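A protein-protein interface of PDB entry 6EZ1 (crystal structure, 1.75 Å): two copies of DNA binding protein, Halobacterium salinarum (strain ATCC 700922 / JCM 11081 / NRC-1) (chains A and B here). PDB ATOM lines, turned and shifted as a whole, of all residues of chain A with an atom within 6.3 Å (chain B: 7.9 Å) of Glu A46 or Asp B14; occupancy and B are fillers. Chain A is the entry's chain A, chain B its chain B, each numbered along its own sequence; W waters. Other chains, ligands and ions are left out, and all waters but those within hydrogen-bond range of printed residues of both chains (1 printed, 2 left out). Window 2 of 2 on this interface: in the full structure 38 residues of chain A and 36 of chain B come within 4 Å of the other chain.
Of the 10 printed residues of chain A, 4 touch a printed residue of chain B.
Printed residues of chain A that touch a printed residue of chain B: Glu A42, Tyr A43, Tyr A44 and Glu A46.
Hydrophobic or aromatic side chains of chain A within 4 Å of the printed part of chain B: Tyr A43 and Tyr A44.
Among the printed residues, 7 pairs touch across the chains.
The side-chain carboxylate of Asp B11 sits at hydrogen-bond distance from the backbone NH of Arg B13 (3.2 Å).
The side-chain amino group of Lys B20 lies within salt-bridge range of the side-chain carboxylate of Asp B91 (2.6 Å).
Of the printed residues of chain A, Arg B13 touches Glu A42 (3.96 Å), Tyr A43 (2.7 Å) and Tyr A44 (3.5 Å).
Of chain A, only Tyr A44 and Glu A46 come within 4 Å of Asp B14.
Of the printed residues of chain A, Asp B91 touches Tyr A43.
The nearest residue of chain B that does not touch Glu A46 is Asp B11 (6.8 Å).
The nearest residue of chain A that does not touch Asp B14 is Tyr A43 (5.6 Å).
The nearest printed residue of chain B that does not touch Tyr A43 is Asp B11 (5.0 Å).
Water W1 lies within hydrogen-bond range of the side-chain carboxylate of Asp B14 (2.6 Å) and the backbone carbonyl oxygen of Tyr A44 (2.6 Å).
The side-chain hydroxyl (OH) of Tyr A43 is in hydrogen-bond range of the side-chain amino group (NZ) of Lys B20, 2.5 Å away.
OD1 of Asp B91 sits at hydrogen-bond distance from OH of Tyr A43, 2.8 Å away.
O of Tyr A43 lies within hydrogen-bond range of NH1 of Arg B13.
The side-chain carboxylate (OE2) of Glu A46 lies close to the side-chain carboxylate (OD2) of Asp B14 (3.5 Å).
Arg B13 touches Glu A42 (NH1 to O, 3.96 Å).
CE1 of Tyr A44 touches O of Arg B13, at 3.5 Å.
CD1 of Tyr A44 touches OD1 of Asp B14, 3.4 Å away.
No position is printed for both chains.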
ATOM      1  N   LYS A  37     -15.649   9.203 -11.969  1.00  0.00           N
ATOM      2  CA  LYS A  37     -15.437   8.671 -13.307  1.00  0.00           C
ATOM      3  C   LYS A  37     -13.956   8.610 -13.643  1.00  0.00           C
ATOM      4  O   LYS A  37     -13.466   7.590 -14.140  1.00  0.00           O
ATOM      5  CB  LYS A  37     -16.195   9.512 -14.333  1.00  0.00           C
ATOM      6  CG  LYS A  37     -16.585   8.726 -15.577  1.00  0.00           C
ATOM      7  CD  LYS A  37     -17.693   9.412 -16.350  1.00  0.00           C
ATOM      8  CE  LYS A  37     -17.122  10.285 -17.458  1.00  0.00           C
ATOM      9  NZ  LYS A  37     -16.349   9.473 -18.448  1.00  0.00           N
ATOM     10  N   LEU A  40     -12.091   5.877 -11.749  1.00  0.00           N
ATOM     11  CA  LEU A  40     -12.321   4.561 -12.329  1.00  0.00           C
ATOM     12  C   LEU A  40     -11.578   4.401 -13.650  1.00  0.00           C
ATOM     13  O   LEU A  40     -11.075   3.311 -13.954  1.00  0.00           O
ATOM     14  CB  LEU A  40     -13.815   4.338 -12.523  1.00  0.00           C
ATOM     15  CG  LEU A  40     -14.638   4.266 -11.239  1.00  0.00           C
ATOM     16  CD1 LEU A  40     -16.118   4.364 -11.602  1.00  0.00           C
ATOM     17  CD2 LEU A  40     -14.352   3.004 -10.466  1.00  0.00           C
ATOM     18  N   GLU A  41     -11.508   5.466 -14.455  1.00  0.00           N
ATOM     19  CA  GLU A  41     -10.782   5.384 -15.717  1.00  0.00           C
ATOM     20  C   GLU A  41      -9.299   5.146 -15.480  1.00  0.00           C
ATOM     21  O   GLU A  41      -8.662   4.382 -16.215  1.00  0.00           O
ATOM     22  CB  GLU A  41     -11.002   6.653 -16.539  1.00  0.00           C
ATOM     23  CG  GLU A  41     -12.393   6.723 -17.131  1.00  0.00           C
ATOM     24  CD  GLU A  41     -12.618   7.919 -18.014  1.00  0.00           C
ATOM     25  OE1 GLU A  41     -11.879   8.926 -17.888  1.00  0.00           O
ATOM     26  OE2 GLU A  41     -13.545   7.863 -18.854  1.00  0.00           O
ATOM     27  N   GLU A  42      -8.727   5.785 -14.461  1.00  0.00           N
ATOM     28  CA  GLU A  42      -7.336   5.514 -14.131  1.00  0.00           C
ATOM     29  C   GLU A  42      -7.148   4.064 -13.702  1.00  0.00           C
ATOM     30  O   GLU A  42      -6.120   3.452 -14.011  1.00  0.00           O
ATOM     31  CB  GLU A  42      -6.852   6.453 -13.032  1.00  0.00           C
ATOM     32  CG  GLU A  42      -5.376   6.282 -12.747  1.00  0.00           C
ATOM     33  CD  GLU A  42      -4.795   7.393 -11.912  1.00  0.00           C
ATOM     34  OE1 GLU A  42      -5.553   8.306 -11.522  1.00  0.00           O
ATOM     35  OE2 GLU A  42      -3.575   7.348 -11.653  1.00  0.00           O
ATOM     36  N   TYR A  43      -8.127   3.502 -12.989  1.00  0.00           N
ATOM     37  CA  TYR A  43      -8.046   2.103 -12.585  1.00  0.00           C
ATOM     38  C   TYR A  43      -8.121   1.179 -13.791  1.00  0.00           C
ATOM     39  O   TYR A  43      -7.257   0.314 -13.979  1.00  0.00           O
ATOM     40  CB  TYR A  43      -9.165   1.774 -11.599  1.00  0.00           C
ATOM     41  CG  TYR A  43      -9.265   0.294 -11.300  1.00  0.00           C
ATOM     42  CD1 TYR A  43      -8.373  -0.319 -10.432  1.00  0.00           C
ATOM     43  CD2 TYR A  43     -10.245  -0.488 -11.894  1.00  0.00           C
ATOM     44  CE1 TYR A  43      -8.456  -1.673 -10.158  1.00  0.00           C
ATOM     45  CE2 TYR A  43     -10.337  -1.839 -11.626  1.00  0.00           C
ATOM     46  CZ  TYR A  43      -9.440  -2.428 -10.761  1.00  0.00           C
ATOM     47  OH  TYR A  43      -9.530  -3.777 -10.494  1.00  0.00           O
ATOM     48  N   TYR A  44      -9.157   1.338 -14.614  1.00  0.00           N
ATOM     49  CA  TYR A  44      -9.373   0.428 -15.727  1.00  0.00           C
ATOM     50  C   TYR A  44      -8.407   0.666 -16.881  1.00  0.00           C
ATOM     51  O   TYR A  44      -8.174  -0.253 -17.675  1.00  0.00           O
ATOM     52  CB  TYR A  44     -10.811   0.552 -16.238  1.00  0.00           C
ATOM     53  CG  TYR A  44     -11.856  -0.026 -15.305  1.00  0.00           C
ATOM     54  CD1 TYR A  44     -11.925  -1.397 -15.072  1.00  0.00           C
ATOM     55  CD2 TYR A  44     -12.777   0.793 -14.664  1.00  0.00           C
ATOM     56  CE1 TYR A  44     -12.874  -1.929 -14.221  1.00  0.00           C
ATOM     57  CE2 TYR A  44     -13.729   0.268 -13.811  1.00  0.00           C
ATOM     58  CZ  TYR A  44     -13.775  -1.092 -13.596  1.00  0.00           C
ATOM     59  OH  TYR A  44     -14.728  -1.609 -12.749  1.00  0.00           O
ATOM     60  N   GLY A  45      -7.841   1.865 -16.994  1.00  0.00           N
ATOM     61  CA  GLY A  45      -7.070   2.193 -18.173  1.00  0.00           C
ATOM     62  C   GLY A  45      -7.914   2.305 -19.416  1.00  0.00           C
ATOM     63  O   GLY A  45      -7.393   2.189 -20.530  1.00  0.00           O
ATOM     64  N   GLU A  46      -9.216   2.517 -19.244  1.00  0.00           N
ATOM     65  CA  GLU A  46     -10.170   2.594 -20.333  1.00  0.00           C
ATOM     66  C   GLU A  46     -11.224   3.625 -19.965  1.00  0.00           C
ATOM     67  O   GLU A  46     -11.467   3.887 -18.785  1.00  0.00           O
ATOM     68  CB  GLU A  46     -10.851   1.245 -20.593  1.00  0.00           C
ATOM     69  CG  GLU A  46      -9.921   0.098 -20.933  1.00  0.00           C
ATOM     70  CD  GLU A  46     -10.634  -1.244 -20.907  1.00  0.00           C
ATOM     71  OE1 GLU A  46     -11.755  -1.325 -20.360  1.00  0.00           O
ATOM     72  OE2 GLU A  46     -10.075  -2.223 -21.437  1.00  0.00           O
ATOM     73  N   GLU A  47     -11.864   4.190 -20.982  1.00  0.00           N
ATOM     74  CA  GLU A  47     -12.934   5.147 -20.744  1.00  0.00           C
ATOM     75  C   GLU A  47     -14.100   4.494 -20.016  1.00  0.00           C
ATOM     76  O   GLU A  47     -14.435   3.330 -20.259  1.00  0.00           O
ATOM     77  CB  GLU A  47     -13.432   5.732 -22.063  1.00  0.00           C
ATOM     78  CG  GLU A  47     -12.480   6.680 -22.733  1.00  0.00           C
ATOM     79  CD  GLU A  47     -13.139   7.401 -23.882  1.00  0.00           C
ATOM     80  OE1 GLU A  47     -13.125   6.861 -25.007  1.00  0.00           O
ATOM     81  OE2 GLU A  47     -13.686   8.500 -23.650  1.00  0.00           O
ATOM     82  N   VAL A  48     -14.729   5.260 -19.131  1.00  0.00           N
ATOM     83  CA  VAL A  48     -15.945   4.850 -18.439  1.00  0.00           C
ATOM     84  C   VAL A  48     -17.064   5.777 -18.890  1.00  0.00           C
ATOM     85  O   VAL A  48     -16.959   7.000 -18.744  1.00  0.00           O
ATOM     86  CB  VAL A  48     -15.774   4.884 -16.914  1.00  0.00           C
ATOM     87  CG1 VAL A  48     -17.100   4.584 -16.229  1.00  0.00           C
ATOM     88  CG2 VAL A  48     -14.708   3.888 -16.486  1.00  0.00           C
ATOM     89  N   ASP B  11      -3.706  -7.635 -18.389  1.00  0.00           N
ATOM     90  CA  ASP B  11      -4.334  -6.880 -17.310  1.00  0.00           C
ATOM     91  C   ASP B  11      -5.686  -7.482 -16.941  1.00  0.00           C
ATOM     92  O   ASP B  11      -6.571  -7.618 -17.789  1.00  0.00           O
ATOM     93  CB  ASP B  11      -4.502  -5.416 -17.709  1.00  0.00           C
ATOM     94  CG  ASP B  11      -4.974  -4.553 -16.558  1.00  0.00           C
ATOM     95  OD1 ASP B  11      -5.097  -5.076 -15.433  1.00  0.00           O
ATOM     96  OD2 ASP B  11      -5.225  -3.351 -16.776  1.00  0.00           O
ATOM     97  N   ALA B  12      -5.843  -7.827 -15.661  1.00  0.00           N
ATOM     98  CA  ALA B  12      -7.024  -8.531 -15.178  1.00  0.00           C
ATOM     99  C   ALA B  12      -7.956  -7.635 -14.371  1.00  0.00           C
ATOM    100  O   ALA B  12      -8.777  -8.139 -13.599  1.00  0.00           O
ATOM    101  CB  ALA B  12      -6.612  -9.740 -14.337  1.00  0.00           C
ATOM    102  N   ARG B  13      -7.856  -6.315 -14.531  1.00  0.00           N
ATOM    103  CA  ARG B  13      -8.743  -5.423 -13.797  1.00  0.00           C
ATOM    104  C   ARG B  13     -10.168  -5.439 -14.337  1.00  0.00           C
ATOM    105  O   ARG B  13     -11.061  -4.875 -13.695  1.00  0.00           O
ATOM    106  CB  ARG B  13      -8.186  -3.998 -13.821  1.00  0.00           C
ATOM    107  CG  ARG B  13      -6.903  -3.844 -13.018  1.00  0.00           C
ATOM    108  CD  ARG B  13      -6.419  -2.403 -12.968  1.00  0.00           C
ATOM    109  NE  ARG B  13      -5.294  -2.253 -12.047  1.00  0.00           N
ATOM    110  CZ  ARG B  13      -4.760  -1.087 -11.694  1.00  0.00           C
ATOM    111  NH1 ARG B  13      -5.252   0.045 -12.182  1.00  0.00           N
ATOM    112  NH2 ARG B  13      -3.736  -1.054 -10.849  1.00  0.00           N
ATOM    113  N   ASP B  14     -10.406  -6.078 -15.480  1.00  0.00           N
ATOM    114  CA  ASP B  14     -11.738  -6.153 -16.068  1.00  0.00           C
ATOM    115  C   ASP B  14     -12.509  -7.397 -15.650  1.00  0.00           C
ATOM    116  O   ASP B  14     -13.637  -7.595 -16.113  1.00  0.00           O
ATOM    117  CB  ASP B  14     -11.636  -6.118 -17.596  1.00  0.00           C
ATOM    118  CG  ASP B  14     -11.109  -4.799 -18.115  1.00  0.00           C
ATOM    119  OD1 ASP B  14     -11.367  -3.763 -17.471  1.00  0.00           O
ATOM    120  OD2 ASP B  14     -10.436  -4.798 -19.166  1.00  0.00           O
ATOM    121  N   LEU B  15     -11.931  -8.240 -14.804  1.00  0.00           N
ATOM    122  CA  LEU B  15     -12.593  -9.471 -14.404  1.00  0.00           C
ATOM    123  C   LEU B  15     -13.859  -9.168 -13.614  1.00  0.00           C
ATOM    124  O   LEU B  15     -13.990  -8.120 -12.981  1.00  0.00           O
ATOM    125  CB  LEU B  15     -11.655 -10.320 -13.550  1.00  0.00           C
ATOM    126  CG  LEU B  15     -10.420 -10.910 -14.217  1.00  0.00           C
ATOM    127  CD1 LEU B  15      -9.565 -11.599 -13.161  1.00  0.00           C
ATOM    128  CD2 LEU B  15     -10.828 -11.871 -15.313  1.00  0.00           C
ATOM    129  N   THR B  16     -14.799 -10.104 -13.650  1.00  0.00           N
ATOM    130  CA  THR B  16     -15.977  -9.979 -12.810  1.00  0.00           C
ATOM    131  C   THR B  16     -15.596 -10.194 -11.348  1.00  0.00           C
ATOM    132  O   THR B  16     -14.575 -10.815 -11.025  1.00  0.00           O
ATOM    133  CB  THR B  16     -17.054 -10.994 -13.206  1.00  0.00           C
ATOM    134  OG1 THR B  16     -16.605 -12.314 -12.878  1.00  0.00           O
ATOM    135  CG2 THR B  16     -17.360 -10.900 -14.690  1.00  0.00           C
ATOM    136  N   ALA B  17     -16.445  -9.685 -10.453  1.00  0.00           N
ATOM    137  CA  ALA B  17     -16.231  -9.908  -9.026  1.00  0.00           C
ATOM    138  C   ALA B  17     -16.141 -11.397  -8.702  1.00  0.00           C
ATOM    139  O   ALA B  17     -15.314 -11.813  -7.883  1.00  0.00           O
ATOM    140  CB  ALA B  17     -17.352  -9.247  -8.224  1.00  0.00           C
ATOM    141  N   GLN B  19     -15.076 -13.861 -10.657  1.00  0.00           N
ATOM    142  CA  GLN B  19     -13.762 -14.333 -11.084  1.00  0.00           C
ATOM    143  C   GLN B  19     -12.668 -13.833 -10.156  1.00  0.00           C
ATOM    144  O   GLN B  19     -11.750 -14.583  -9.807  1.00  0.00           O
ATOM    145  CB  GLN B  19     -13.489 -13.890 -12.521  1.00  0.00           C
ATOM    146  CG  GLN B  19     -14.423 -14.559 -13.512  1.00  0.00           C
ATOM    147  CD  GLN B  19     -14.348 -13.986 -14.904  1.00  0.00           C
ATOM    148  OE1 GLN B  19     -14.068 -12.800 -15.091  1.00  0.00           O
ATOM    149  NE2 GLN B  19     -14.626 -14.821 -15.898  1.00  0.00           N
ATOM    150  N   LYS B  20     -12.739 -12.565  -9.754  1.00  0.00           N
ATOM    151  CA  LYS B  20     -11.759 -12.031  -8.819  1.00  0.00           C
ATOM    152  C   LYS B  20     -11.817 -12.761  -7.483  1.00  0.00           C
ATOM    153  O   LYS B  20     -10.783 -12.950  -6.834  1.00  0.00           O
ATOM    154  CB  LYS B  20     -11.984 -10.526  -8.640  1.00  0.00           C
ATOM    155  CG  LYS B  20     -11.672  -9.703  -9.893  1.00  0.00           C
ATOM    156  CD  LYS B  20     -11.537  -8.221  -9.567  1.00  0.00           C
ATOM    157  CE  LYS B  20     -11.126  -7.410 -10.787  1.00  0.00           C
ATOM    158  NZ  LYS B  20     -10.616  -6.061 -10.402  1.00  0.00           N
ATOM    159  N   LYS B  63      -7.275 -17.448 -19.702  1.00  0.00           N
ATOM    160  CA  LYS B  63      -6.629 -16.155 -19.534  1.00  0.00           C
ATOM    161  C   LYS B  63      -5.224 -16.270 -18.957  1.00  0.00           C
ATOM    162  O   LYS B  63      -4.533 -15.252 -18.849  1.00  0.00           O
ATOM    163  CB  LYS B  63      -7.475 -15.256 -18.630  1.00  0.00           C
ATOM    164  CG  LYS B  63      -8.797 -14.809 -19.231  1.00  0.00           C
ATOM    165  CD  LYS B  63      -9.651 -14.110 -18.186  1.00  0.00           C
ATOM    166  CE  LYS B  63     -10.979 -13.650 -18.765  1.00  0.00           C
ATOM    167  NZ  LYS B  63     -10.813 -12.484 -19.683  1.00  0.00           N
ATOM    168  N   ASP B  91      -4.756  -5.825  -7.425  1.00  0.00           N
ATOM    169  CA  ASP B  91      -6.041  -5.366  -6.905  1.00  0.00           C
ATOM    170  C   ASP B  91      -5.937  -4.983  -5.434  1.00  0.00           C
ATOM    171  O   ASP B  91      -6.534  -3.991  -5.002  1.00  0.00           O
ATOM    172  CB  ASP B  91      -7.094  -6.455  -7.100  1.00  0.00           C
ATOM    173  CG  ASP B  91      -8.392  -5.915  -7.662  1.00  0.00           C
ATOM    174  OD1 ASP B  91      -8.492  -5.771  -8.898  1.00  0.00           O
ATOM    175  OD2 ASP B  91      -9.310  -5.619  -6.870  1.00  0.00           O
HETATM  176  O   HOH W   1      -9.022  -2.706 -17.411  1.00  0.00           O
